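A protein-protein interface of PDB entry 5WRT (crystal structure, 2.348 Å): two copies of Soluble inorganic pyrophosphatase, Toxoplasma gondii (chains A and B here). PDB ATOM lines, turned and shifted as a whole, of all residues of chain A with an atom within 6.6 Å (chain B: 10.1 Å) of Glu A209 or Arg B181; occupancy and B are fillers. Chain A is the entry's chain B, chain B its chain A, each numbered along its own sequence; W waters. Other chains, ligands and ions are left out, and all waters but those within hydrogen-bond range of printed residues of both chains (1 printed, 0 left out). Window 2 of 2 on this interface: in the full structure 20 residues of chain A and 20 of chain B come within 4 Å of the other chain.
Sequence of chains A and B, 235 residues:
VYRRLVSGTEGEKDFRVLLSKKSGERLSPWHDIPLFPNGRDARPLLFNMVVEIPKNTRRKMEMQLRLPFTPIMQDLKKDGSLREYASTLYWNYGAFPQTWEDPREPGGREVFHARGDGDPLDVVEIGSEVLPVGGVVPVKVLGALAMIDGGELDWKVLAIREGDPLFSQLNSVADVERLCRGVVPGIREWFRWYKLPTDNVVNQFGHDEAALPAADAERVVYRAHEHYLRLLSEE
The guanidinium group of Arg B181 lies close to the side-chain carboxylate of Glu A209, at 2.4 Å. The side-chain carboxylate (OE1) of Glu A189 lies close to the backbone carbonyl oxygen (O) of Gly B182 (3.3 Å). The indole nitrogen of Trp A193 lies within hydrogen-bond range of the backbone carbonyl oxygen of Gly B182, at 3.1 Å.
1 position is printed for both chains. Of the 10 pairs that touch across the chains among the printed residues, none has its exchanged pair printed and touching as well.
Of the 19 printed residues of chain B, 6 touch a printed residue of chain A. Hydrophobic or aromatic side chains of chain B that line the printed part of chain A: Trp B91 and Pro B185. Along chain B the printed residues that touch a printed residue of chain A span positions 91 to 186.
Water W1 lies within hydrogen-bond range of the side-chain carboxylate of Glu A209, the backbone NH of Phe A205 and the guanidinium group of Arg B181.
OE1 of Glu A189 sits at hydrogen-bond distance from NE1 of Trp A193, 3.1 Å away. The backbone carbonyl oxygen of Arg A192 lies within hydrogen-bond range of the backbone NH of Asn A203, at 3.1 Å. The side-chain carboxylate (OE2) of Glu A209 is in salt-bridge range of the guanidinium group (NH1) of Arg A192 (2.9 Å). OE1 of Glu A189 is in salt-bridge range of NE of Arg A192, at 2.8 Å. The guanidinium group of Arg A188 sits at hydrogen-bond distance from the backbone carbonyl oxygen of Glu A209.
Glu A209 touches just one residue of chain B: Arg B181 (2.4 Å). Arg B181 touches two residues of chain A. No residue of chain B comes within 4 Å of Gly A206. Asp A208 touches none of the printed residues of chain B. No residue of chain B comes within 4 Å of Ala A210. Printed residues of chain A within 4 Å of Val B183: Trp A193. Printed residues of chain B within 4 Å of Arg A192: Arg B181 (3.8 Å) and Gly B182 (3.5 Å). Printed residues of chain A within 4 Å of Trp B91: Trp A193. Printed residues of chain B within 4 Å of Trp A193: Trp B91 (3.8 Å), Gly B182 (3.1 Å), Val B183 (3.9 Å) and Gly B186 (3.7 Å). Of the printed residues of chain A, Gly B182 touches Glu A189, Arg A192 and Trp A193. Leu A145 touches none of the printed residues of chain B. Val A202 touches none of the printed residues of chain B. The nearest residue of chain A that does not touch Arg B181 is Trp A193 (4.5 Å).
Among the printed residues, merely in contact across the chains: Glu A189 with Pro B185 (3.4 Å), Glu A189 with Gly B186 (3.6 Å), Arg A192 with Arg B181 (3.8 Å), Arg A192 with Gly B182 (3.5 Å), Trp A193 with Trp B91 (3.8 Å), Trp A193 with Val B183 (3.9 Å) and Trp A193 with Gly B186 (3.7 Å).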
ATOM      1  N   LEU A 145      37.717  19.962  -9.960  1.00  0.00           N
ATOM      2  CA  LEU A 145      37.095  19.301  -8.822  1.00  0.00           C
ATOM      3  C   LEU A 145      38.043  18.232  -8.299  1.00  0.00           C
ATOM      4  O   LEU A 145      38.594  17.450  -9.082  1.00  0.00           O
ATOM      5  CB  LEU A 145      35.755  18.678  -9.217  1.00  0.00           C
ATOM      6  CG  LEU A 145      34.617  19.650  -9.537  1.00  0.00           C
ATOM      7  CD1 LEU A 145      33.590  18.983 -10.436  1.00  0.00           C
ATOM      8  CD2 LEU A 145      33.968  20.154  -8.258  1.00  0.00           C
ATOM      9  N   ALA A 146      38.237  18.201  -6.981  1.00  0.00           N
ATOM     10  CA  ALA A 146      39.184  17.279  -6.355  1.00  0.00           C
ATOM     11  C   ALA A 146      38.433  16.053  -5.842  1.00  0.00           C
ATOM     12  O   ALA A 146      38.144  15.921  -4.654  1.00  0.00           O
ATOM     13  CB  ALA A 146      39.951  17.975  -5.235  1.00  0.00           C
ATOM     14  N   VAL A 184      28.660  22.612 -13.461  1.00  0.00           N
ATOM     15  CA  VAL A 184      29.558  22.340 -12.336  1.00  0.00           C
ATOM     16  C   VAL A 184      28.945  21.351 -11.348  1.00  0.00           C
ATOM     17  O   VAL A 184      29.599  20.342 -11.037  1.00  0.00           O
ATOM     18  CB  VAL A 184      29.999  23.657 -11.675  1.00  0.00           C
ATOM     19  CG1 VAL A 184      30.829  23.371 -10.429  1.00  0.00           C
ATOM     20  CG2 VAL A 184      30.782  24.512 -12.657  1.00  0.00           C
ATOM     21  N   ARG A 188      30.058  17.373 -10.727  1.00  0.00           N
ATOM     22  CA  ARG A 188      30.379  16.935  -9.371  1.00  0.00           C
ATOM     23  C   ARG A 188      29.492  15.772  -8.944  1.00  0.00           C
ATOM     24  O   ARG A 188      29.977  14.769  -8.410  1.00  0.00           O
ATOM     25  CB  ARG A 188      30.242  18.102  -8.393  1.00  0.00           C
ATOM     26  CG  ARG A 188      30.506  17.726  -6.941  1.00  0.00           C
ATOM     27  CD  ARG A 188      30.514  18.952  -6.040  1.00  0.00           C
ATOM     28  NE  ARG A 188      29.610  19.985  -6.533  1.00  0.00           N
ATOM     29  CZ  ARG A 188      29.957  21.251  -6.733  1.00  0.00           C
ATOM     30  NH1 ARG A 188      31.193  21.656  -6.469  1.00  0.00           N
ATOM     31  NH2 ARG A 188      29.064  22.116  -7.189  1.00  0.00           N
ATOM     32  N   GLU A 189      28.180  15.890  -9.168  1.00  0.00           N
ATOM     33  CA  GLU A 189      27.272  14.825  -8.753  1.00  0.00           C
ATOM     34  C   GLU A 189      27.423  13.577  -9.616  1.00  0.00           C
ATOM     35  O   GLU A 189      27.198  12.465  -9.127  1.00  0.00           O
ATOM     36  CB  GLU A 189      25.825  15.317  -8.777  1.00  0.00           C
ATOM     37  CG  GLU A 189      25.504  16.393  -7.741  1.00  0.00           C
ATOM     38  CD  GLU A 189      26.008  16.052  -6.346  1.00  0.00           C
ATOM     39  OE1 GLU A 189      25.923  14.872  -5.942  1.00  0.00           O
ATOM     40  OE2 GLU A 189      26.483  16.970  -5.645  1.00  0.00           O
ATOM     41  N   ARG A 192      30.375  11.842  -8.192  1.00  0.00           N
ATOM     42  CA  ARG A 192      30.121  11.423  -6.817  1.00  0.00           C
ATOM     43  C   ARG A 192      29.356  10.105  -6.772  1.00  0.00           C
ATOM     44  O   ARG A 192      29.605   9.267  -5.898  1.00  0.00           O
ATOM     45  CB  ARG A 192      29.353  12.506  -6.059  1.00  0.00           C
ATOM     46  CG  ARG A 192      29.301  12.261  -4.555  1.00  0.00           C
ATOM     47  CD  ARG A 192      28.016  12.774  -3.922  1.00  0.00           C
ATOM     48  NE  ARG A 192      27.850  14.213  -4.091  1.00  0.00           N
ATOM     49  CZ  ARG A 192      28.402  15.124  -3.297  1.00  0.00           C
ATOM     50  NH1 ARG A 192      29.159  14.744  -2.277  1.00  0.00           N
ATOM     51  NH2 ARG A 192      28.198  16.414  -3.523  1.00  0.00           N
ATOM     52  N   TRP A 193      28.423   9.903  -7.705  1.00  0.00           N
ATOM     53  CA  TRP A 193      27.453   8.821  -7.617  1.00  0.00           C
ATOM     54  C   TRP A 193      27.684   7.673  -8.591  1.00  0.00           C
ATOM     55  O   TRP A 193      27.067   6.614  -8.418  1.00  0.00           O
ATOM     56  CB  TRP A 193      26.036   9.367  -7.838  1.00  0.00           C
ATOM     57  CG  TRP A 193      25.539  10.218  -6.716  1.00  0.00           C
ATOM     58  CD1 TRP A 193      25.501  11.581  -6.674  1.00  0.00           C
ATOM     59  CD2 TRP A 193      25.015   9.762  -5.464  1.00  0.00           C
ATOM     60  NE1 TRP A 193      24.981  12.002  -5.474  1.00  0.00           N
ATOM     61  CE2 TRP A 193      24.676  10.905  -4.712  1.00  0.00           C
ATOM     62  CE3 TRP A 193      24.799   8.497  -4.906  1.00  0.00           C
ATOM     63  CZ2 TRP A 193      24.133  10.822  -3.432  1.00  0.00           C
ATOM     64  CZ3 TRP A 193      24.259   8.418  -3.635  1.00  0.00           C
ATOM     65  CH2 TRP A 193      23.933   9.572  -2.912  1.00  0.00           C
ATOM     66  N   VAL A 202      30.011   5.959  -2.418  1.00  0.00           N
ATOM     67  CA  VAL A 202      29.793   7.363  -2.747  1.00  0.00           C
ATOM     68  C   VAL A 202      31.119   8.083  -2.554  1.00  0.00           C
ATOM     69  O   VAL A 202      31.684   8.073  -1.454  1.00  0.00           O
ATOM     70  CB  VAL A 202      28.690   7.988  -1.881  1.00  0.00           C
ATOM     71  CG1 VAL A 202      28.523   9.460  -2.219  1.00  0.00           C
ATOM     72  CG2 VAL A 202      27.379   7.246  -2.077  1.00  0.00           C
ATOM     73  N   ASN A 203      31.616   8.703  -3.619  1.00  0.00           N
ATOM     74  CA  ASN A 203      32.905   9.374  -3.568  1.00  0.00           C
ATOM     75  C   ASN A 203      32.804  10.701  -2.819  1.00  0.00           C
ATOM     76  O   ASN A 203      31.721  11.257  -2.621  1.00  0.00           O
ATOM     77  CB  ASN A 203      33.446   9.601  -4.979  1.00  0.00           C
ATOM     78  CG  ASN A 203      33.722   8.303  -5.712  1.00  0.00           C
ATOM     79  OD1 ASN A 203      34.448   7.441  -5.215  1.00  0.00           O
ATOM     80  ND2 ASN A 203      33.145   8.157  -6.899  1.00  0.00           N
ATOM     81  N   GLN A 204      33.959  11.204  -2.398  1.00  0.00           N
ATOM     82  CA  GLN A 204      34.072  12.504  -1.753  1.00  0.00           C
ATOM     83  C   GLN A 204      34.812  13.476  -2.662  1.00  0.00           C
ATOM     84  O   GLN A 204      35.380  13.099  -3.692  1.00  0.00           O
ATOM     85  CB  GLN A 204      34.803  12.401  -0.409  1.00  0.00           C
ATOM     86  CG  GLN A 204      34.293  11.327   0.528  1.00  0.00           C
ATOM     87  CD  GLN A 204      35.187  11.169   1.743  1.00  0.00           C
ATOM     88  OE1 GLN A 204      36.315  10.686   1.640  1.00  0.00           O
ATOM     89  NE2 GLN A 204      34.691  11.590   2.903  1.00  0.00           N
ATOM     90  N   PHE A 205      34.799  14.745  -2.263  1.00  0.00           N
ATOM     91  CA  PHE A 205      35.523  15.794  -2.965  1.00  0.00           C
ATOM     92  C   PHE A 205      36.309  16.614  -1.955  1.00  0.00           C
ATOM     93  O   PHE A 205      35.768  17.013  -0.919  1.00  0.00           O
ATOM     94  CB  PHE A 205      34.572  16.688  -3.766  1.00  0.00           C
ATOM     95  CG  PHE A 205      33.952  16.000  -4.945  1.00  0.00           C
ATOM     96  CD1 PHE A 205      32.783  15.271  -4.802  1.00  0.00           C
ATOM     97  CD2 PHE A 205      34.544  16.071  -6.196  1.00  0.00           C
ATOM     98  CE1 PHE A 205      32.215  14.631  -5.886  1.00  0.00           C
ATOM     99  CE2 PHE A 205      33.980  15.433  -7.283  1.00  0.00           C
ATOM    100  CZ  PHE A 205      32.814  14.712  -7.128  1.00  0.00           C
ATOM    101  N   GLY A 206      37.577  16.862  -2.260  1.00  0.00           N
ATOM    102  CA  GLY A 206      38.398  17.713  -1.431  1.00  0.00           C
ATOM    103  C   GLY A 206      38.031  19.179  -1.577  1.00  0.00           C
ATOM    104  O   GLY A 206      37.174  19.572  -2.370  1.00  0.00           O
ATOM    105  N   HIS A 207      38.711  20.004  -0.778  1.00  0.00           N
ATOM    106  CA  HIS A 207      38.519  21.455  -0.788  1.00  0.00           C
ATOM    107  C   HIS A 207      37.057  21.829  -0.563  1.00  0.00           C
ATOM    108  O   HIS A 207      36.535  22.761  -1.179  1.00  0.00           O
ATOM    109  CB  HIS A 207      39.041  22.068  -2.091  1.00  0.00           C
ATOM    110  CG  HIS A 207      40.515  21.900  -2.288  1.00  0.00           C
ATOM    111  ND1 HIS A 207      41.439  22.795  -1.795  1.00  0.00           N
ATOM    112  CD2 HIS A 207      41.226  20.935  -2.920  1.00  0.00           C
ATOM    113  CE1 HIS A 207      42.655  22.393  -2.118  1.00  0.00           C
ATOM    114  NE2 HIS A 207      42.554  21.266  -2.800  1.00  0.00           N
ATOM    115  N   ASP A 208      36.389  21.092   0.329  1.00  0.00           N
ATOM    116  CA  ASP A 208      34.985  21.328   0.674  1.00  0.00           C
ATOM    117  C   ASP A 208      34.078  21.245  -0.556  1.00  0.00           C
ATOM    118  O   ASP A 208      33.099  21.986  -0.674  1.00  0.00           O
ATOM    119  CB  ASP A 208      34.815  22.674   1.388  1.00  0.00           C
ATOM    120  CG  ASP A 208      33.462  22.818   2.060  1.00  0.00           C
ATOM    121  OD1 ASP A 208      32.832  23.887   1.903  1.00  0.00           O
ATOM    122  OD2 ASP A 208      33.023  21.860   2.734  1.00  0.00           O
ATOM    123  N   GLU A 209      34.412  20.349  -1.487  1.00  0.00           N
ATOM    124  CA  GLU A 209      33.660  20.070  -2.710  1.00  0.00           C
ATOM    125  C   GLU A 209      33.657  21.237  -3.685  1.00  0.00           C
ATOM    126  O   GLU A 209      32.961  21.179  -4.708  1.00  0.00           O
ATOM    127  CB  GLU A 209      32.213  19.652  -2.420  1.00  0.00           C
ATOM    128  CG  GLU A 209      32.072  18.556  -1.381  1.00  0.00           C
ATOM    129  CD  GLU A 209      30.734  17.849  -1.464  1.00  0.00           C
ATOM    130  OE1 GLU A 209      29.816  18.383  -2.124  1.00  0.00           O
ATOM    131  OE2 GLU A 209      30.599  16.762  -0.867  1.00  0.00           O
ATOM    132  N   ALA A 210      34.407  22.298  -3.403  1.00  0.00           N
ATOM    133  CA  ALA A 210      34.434  23.454  -4.284  1.00  0.00           C
ATOM    134  C   ALA A 210      35.194  23.141  -5.568  1.00  0.00           C
ATOM    135  O   ALA A 210      36.114  22.319  -5.591  1.00  0.00           O
ATOM    136  CB  ALA A 210      35.070  24.651  -3.578  1.00  0.00           C
ATOM    137  N   ALA A 211      34.787  23.798  -6.649  1.00  0.00           N
ATOM    138  CA  ALA A 211      35.567  23.812  -7.882  1.00  0.00           C
ATOM    139  C   ALA A 211      36.667  24.857  -7.748  1.00  0.00           C
ATOM    140  O   ALA A 211      36.382  26.057  -7.668  1.00  0.00           O
ATOM    141  CB  ALA A 211      34.670  24.103  -9.083  1.00  0.00           C
ATOM    142  N   TRP B  91      18.430   5.866  -6.727  1.00  0.00           N
ATOM    143  CA  TRP B  91      17.482   5.872  -5.624  1.00  0.00           C
ATOM    144  C   TRP B  91      16.216   5.145  -6.044  1.00  0.00           C
ATOM    145  O   TRP B  91      15.872   5.103  -7.229  1.00  0.00           O
ATOM    146  CB  TRP B  91      17.151   7.304  -5.178  1.00  0.00           C
ATOM    147  CG  TRP B  91      18.369   8.145  -4.935  1.00  0.00           C
ATOM    148  CD1 TRP B  91      19.042   8.295  -3.757  1.00  0.00           C
ATOM    149  CD2 TRP B  91      19.074   8.937  -5.901  1.00  0.00           C
ATOM    150  NE1 TRP B  91      20.116   9.133  -3.927  1.00  0.00           N
ATOM    151  CE2 TRP B  91      20.157   9.542  -5.235  1.00  0.00           C
ATOM    152  CE3 TRP B  91      18.890   9.195  -7.263  1.00  0.00           C
ATOM    153  CZ2 TRP B  91      21.053  10.390  -5.885  1.00  0.00           C
ATOM    154  CZ3 TRP B  91      19.781  10.037  -7.906  1.00  0.00           C
ATOM    155  CH2 TRP B  91      20.849  10.625  -7.217  1.00  0.00           C
ATOM    156  N   ILE B 126      14.945   8.010  -0.668  1.00  0.00           N
ATOM    157  CA  ILE B 126      16.381   8.222  -0.536  1.00  0.00           C
ATOM    158  C   ILE B 126      17.026   7.232   0.429  1.00  0.00           C
ATOM    159  O   ILE B 126      18.214   7.364   0.743  1.00  0.00           O
ATOM    160  CB  ILE B 126      16.682   9.669  -0.119  1.00  0.00           C
ATOM    161  CG1 ILE B 126      16.181   9.931   1.301  1.00  0.00           C
ATOM    162  CG2 ILE B 126      16.036  10.646  -1.092  1.00  0.00           C
ATOM    163  CD1 ILE B 126      16.593  11.276   1.853  1.00  0.00           C
ATOM    164  N   LEU B 166      17.444   6.384   9.352  1.00  0.00           N
ATOM    165  CA  LEU B 166      17.409   7.830   9.528  1.00  0.00           C
ATOM    166  C   LEU B 166      16.000   8.413   9.475  1.00  0.00           C
ATOM    167  O   LEU B 166      15.859   9.638   9.400  1.00  0.00           O
ATOM    168  CB  LEU B 166      18.270   8.508   8.463  1.00  0.00           C
ATOM    169  CG  LEU B 166      19.733   8.090   8.332  1.00  0.00           C
ATOM    170  CD1 LEU B 166      20.343   8.683   7.069  1.00  0.00           C
ATOM    171  CD2 LEU B 166      20.516   8.533   9.555  1.00  0.00           C
ATOM    172  N   LEU B 170      15.151  12.526   9.834  1.00  0.00           N
ATOM    173  CA  LEU B 170      14.933  13.308   8.624  1.00  0.00           C
ATOM    174  C   LEU B 170      13.499  13.819   8.604  1.00  0.00           C
ATOM    175  O   LEU B 170      12.556  13.024   8.582  1.00  0.00           O
ATOM    176  CB  LEU B 170      15.222  12.475   7.373  1.00  0.00           C
ATOM    177  CG  LEU B 170      16.632  11.900   7.242  1.00  0.00           C
ATOM    178  CD1 LEU B 170      16.729  10.993   6.023  1.00  0.00           C
ATOM    179  CD2 LEU B 170      17.666  13.014   7.172  1.00  0.00           C
ATOM    180  N   VAL B 173      14.317  19.122   4.014  1.00  0.00           N
ATOM    181  CA  VAL B 173      15.492  19.207   3.147  1.00  0.00           C
ATOM    182  C   VAL B 173      16.754  19.467   3.960  1.00  0.00           C
ATOM    183  O   VAL B 173      17.813  18.886   3.693  1.00  0.00           O
ATOM    184  CB  VAL B 173      15.282  20.295   2.078  1.00  0.00           C
ATOM    185  CG1 VAL B 173      16.537  20.460   1.231  1.00  0.00           C
ATOM    186  CG2 VAL B 173      14.080  19.960   1.207  1.00  0.00           C
ATOM    187  N   ALA B 174      16.663  20.350   4.958  1.00  0.00           N
ATOM    188  CA  ALA B 174      17.846  20.728   5.725  1.00  0.00           C
ATOM    189  C   ALA B 174      18.479  19.525   6.411  1.00  0.00           C
ATOM    190  O   ALA B 174      19.710  19.423   6.488  1.00  0.00           O
ATOM    191  CB  ALA B 174      17.479  21.802   6.751  1.00  0.00           C
ATOM    192  N   ASP B 175      17.659  18.601   6.921  1.00  0.00           N
ATOM    193  CA  ASP B 175      18.202  17.390   7.531  1.00  0.00           C
ATOM    194  C   ASP B 175      18.905  16.517   6.499  1.00  0.00           C
ATOM    195  O   ASP B 175      19.932  15.897   6.799  1.00  0.00           O
ATOM    196  CB  ASP B 175      17.093  16.609   8.234  1.00  0.00           C
ATOM    197  CG  ASP B 175      16.452  17.394   9.360  1.00  0.00           C
ATOM    198  OD1 ASP B 175      17.162  18.187  10.013  1.00  0.00           O
ATOM    199  OD2 ASP B 175      15.238  17.216   9.595  1.00  0.00           O
ATOM    200  N   VAL B 176      18.365  16.450   5.280  1.00  0.00           N
ATOM    201  CA  VAL B 176      19.000  15.662   4.229  1.00  0.00           C
ATOM    202  C   VAL B 176      20.346  16.268   3.854  1.00  0.00           C
ATOM    203  O   VAL B 176      21.356  15.562   3.753  1.00  0.00           O
ATOM    204  CB  VAL B 176      18.070  15.548   3.007  1.00  0.00           C
ATOM    205  CG1 VAL B 176      18.711  14.684   1.930  1.00  0.00           C
ATOM    206  CG2 VAL B 176      16.718  14.989   3.418  1.00  0.00           C
ATOM    207  N   GLU B 177      20.377  17.584   3.635  1.00  0.00           N
ATOM    208  CA  GLU B 177      21.639  18.263   3.355  1.00  0.00           C
ATOM    209  C   GLU B 177      22.654  18.048   4.474  1.00  0.00           C
ATOM    210  O   GLU B 177      23.863  18.008   4.215  1.00  0.00           O
ATOM    211  CB  GLU B 177      21.392  19.758   3.142  1.00  0.00           C
ATOM    212  CG  GLU B 177      20.589  20.113   1.886  1.00  0.00           C
ATOM    213  CD  GLU B 177      21.370  19.984   0.584  1.00  0.00           C
ATOM    214  OE1 GLU B 177      21.031  20.712  -0.373  1.00  0.00           O
ATOM    215  OE2 GLU B 177      22.314  19.168   0.509  1.00  0.00           O
ATOM    216  N   ARG B 178      22.184  17.904   5.716  1.00  0.00           N
ATOM    217  CA  ARG B 178      23.085  17.771   6.856  1.00  0.00           C
ATOM    218  C   ARG B 178      23.589  16.342   7.016  1.00  0.00           C
ATOM    219  O   ARG B 178      24.789  16.117   7.209  1.00  0.00           O
ATOM    220  CB  ARG B 178      22.385  18.224   8.139  1.00  0.00           C
ATOM    221  CG  ARG B 178      23.306  18.322   9.346  1.00  0.00           C
ATOM    222  CD  ARG B 178      22.646  19.045  10.512  1.00  0.00           C
ATOM    223  NE  ARG B 178      21.254  18.643  10.704  1.00  0.00           N
ATOM    224  CZ  ARG B 178      20.869  17.580  11.403  1.00  0.00           C
ATOM    225  NH1 ARG B 178      21.772  16.801  11.985  1.00  0.00           N
ATOM    226  NH2 ARG B 178      19.579  17.295  11.523  1.00  0.00           N
ATOM    227  N   LEU B 179      22.687  15.363   6.941  1.00  0.00           N
ATOM    228  CA  LEU B 179      23.021  13.981   7.252  1.00  0.00           C
ATOM    229  C   LEU B 179      23.252  13.111   6.024  1.00  0.00           C
ATOM    230  O   LEU B 179      23.673  11.960   6.177  1.00  0.00           O
ATOM    231  CB  LEU B 179      21.910  13.353   8.105  1.00  0.00           C
ATOM    232  CG  LEU B 179      21.578  14.057   9.420  1.00  0.00           C
ATOM    233  CD1 LEU B 179      20.297  13.495  10.011  1.00  0.00           C
ATOM    234  CD2 LEU B 179      22.728  13.915  10.401  1.00  0.00           C
ATOM    235  N   CYS B 180      22.987  13.624   4.809  1.00  0.00           N
ATOM    236  CA  CYS B 180      23.133  12.850   3.571  1.00  0.00           C
ATOM    237  C   CYS B 180      23.653  13.789   2.482  1.00  0.00           C
ATOM    238  O   CYS B 180      22.903  14.234   1.610  1.00  0.00           O
ATOM    239  CB  CYS B 180      21.812  12.202   3.156  1.00  0.00           C
ATOM    240  SG  CYS B 180      20.960  11.261   4.435  1.00  0.00           S
ATOM    241  N   ARG B 181      24.948  14.090   2.531  1.00  0.00           N
ATOM    242  CA  ARG B 181      25.516  15.035   1.579  1.00  0.00           C
ATOM    243  C   ARG B 181      25.449  14.480   0.162  1.00  0.00           C
ATOM    244  O   ARG B 181      25.708  13.297  -0.075  1.00  0.00           O
ATOM    245  CB  ARG B 181      26.964  15.361   1.948  1.00  0.00           C
ATOM    246  CG  ARG B 181      27.663  16.247   0.929  1.00  0.00           C
ATOM    247  CD  ARG B 181      28.036  17.598   1.517  1.00  0.00           C
ATOM    248  NE  ARG B 181      28.875  17.456   2.702  1.00  0.00           N
ATOM    249  CZ  ARG B 181      30.146  17.066   2.679  1.00  0.00           C
ATOM    250  NH1 ARG B 181      30.739  16.782   1.526  1.00  0.00           N
ATOM    251  NH2 ARG B 181      30.828  16.964   3.811  1.00  0.00           N
ATOM    252  N   GLY B 182      25.095  15.350  -0.784  1.00  0.00           N
ATOM    253  CA  GLY B 182      25.009  14.984  -2.178  1.00  0.00           C
ATOM    254  C   GLY B 182      23.706  14.354  -2.613  1.00  0.00           C
ATOM    255  O   GLY B 182      23.520  14.132  -3.816  1.00  0.00           O
ATOM    256  N   VAL B 183      22.791  14.063  -1.687  1.00  0.00           N
ATOM    257  CA  VAL B 183      21.541  13.413  -2.071  1.00  0.00           C
ATOM    258  C   VAL B 183      20.634  14.389  -2.811  1.00  0.00           C
ATOM    259  O   VAL B 183      20.156  14.099  -3.914  1.00  0.00           O
ATOM    260  CB  VAL B 183      20.843  12.812  -0.839  1.00  0.00           C
ATOM    261  CG1 VAL B 183      19.413  12.424  -1.182  1.00  0.00           C
ATOM    262  CG2 VAL B 183      21.616  11.599  -0.349  1.00  0.00           C
ATOM    263  N   VAL B 184      20.382  15.559  -2.218  1.00  0.00           N
ATOM    264  CA  VAL B 184      19.536  16.553  -2.881  1.00  0.00           C
ATOM    265  C   VAL B 184      20.144  17.034  -4.195  1.00  0.00           C
ATOM    266  O   VAL B 184      19.442  17.000  -5.220  1.00  0.00           O
ATOM    267  CB  VAL B 184      19.214  17.708  -1.914  1.00  0.00           C
ATOM    268  CG1 VAL B 184      18.463  18.809  -2.645  1.00  0.00           C
ATOM    269  CG2 VAL B 184      18.399  17.200  -0.736  1.00  0.00           C
ATOM    270  N   PRO B 185      21.405  17.483  -4.252  1.00  0.00           N
ATOM    271  CA  PRO B 185      21.958  17.874  -5.559  1.00  0.00           C
ATOM    272  C   PRO B 185      22.123  16.703  -6.509  1.00  0.00           C
ATOM    273  O   PRO B 185      21.990  16.886  -7.726  1.00  0.00           O
ATOM    274  CB  PRO B 185      23.308  18.509  -5.199  1.00  0.00           C
ATOM    275  CG  PRO B 185      23.677  17.897  -3.905  1.00  0.00           C
ATOM    276  CD  PRO B 185      22.389  17.682  -3.169  1.00  0.00           C
ATOM    277  N   GLY B 186      22.404  15.503  -5.997  1.00  0.00           N
ATOM    278  CA  GLY B 186      22.490  14.346  -6.871  1.00  0.00           C
ATOM    279  C   GLY B 186      21.180  14.055  -7.579  1.00  0.00           C
ATOM    280  O   GLY B 186      21.167  13.719  -8.765  1.00  0.00           O
ATOM    281  N   ILE B 187      20.060  14.195  -6.866  1.00  0.00           N
ATOM    282  CA  ILE B 187      18.755  13.978  -7.483  1.00  0.00           C
ATOM    283  C   ILE B 187      18.433  15.093  -8.471  1.00  0.00           C
ATOM    284  O   ILE B 187      17.934  14.836  -9.573  1.00  0.00           O
ATOM    285  CB  ILE B 187      17.668  13.847  -6.399  1.00  0.00           C
ATOM    286  CG1 ILE B 187      17.833  12.533  -5.636  1.00  0.00           C
ATOM    287  CG2 ILE B 187      16.278  13.943  -7.015  1.00  0.00           C
ATOM    288  CD1 ILE B 187      17.084  12.496  -4.322  1.00  0.00           C
HETATM  289  O   HOH W   1      32.742  15.210  -0.234  1.00  0.00           O
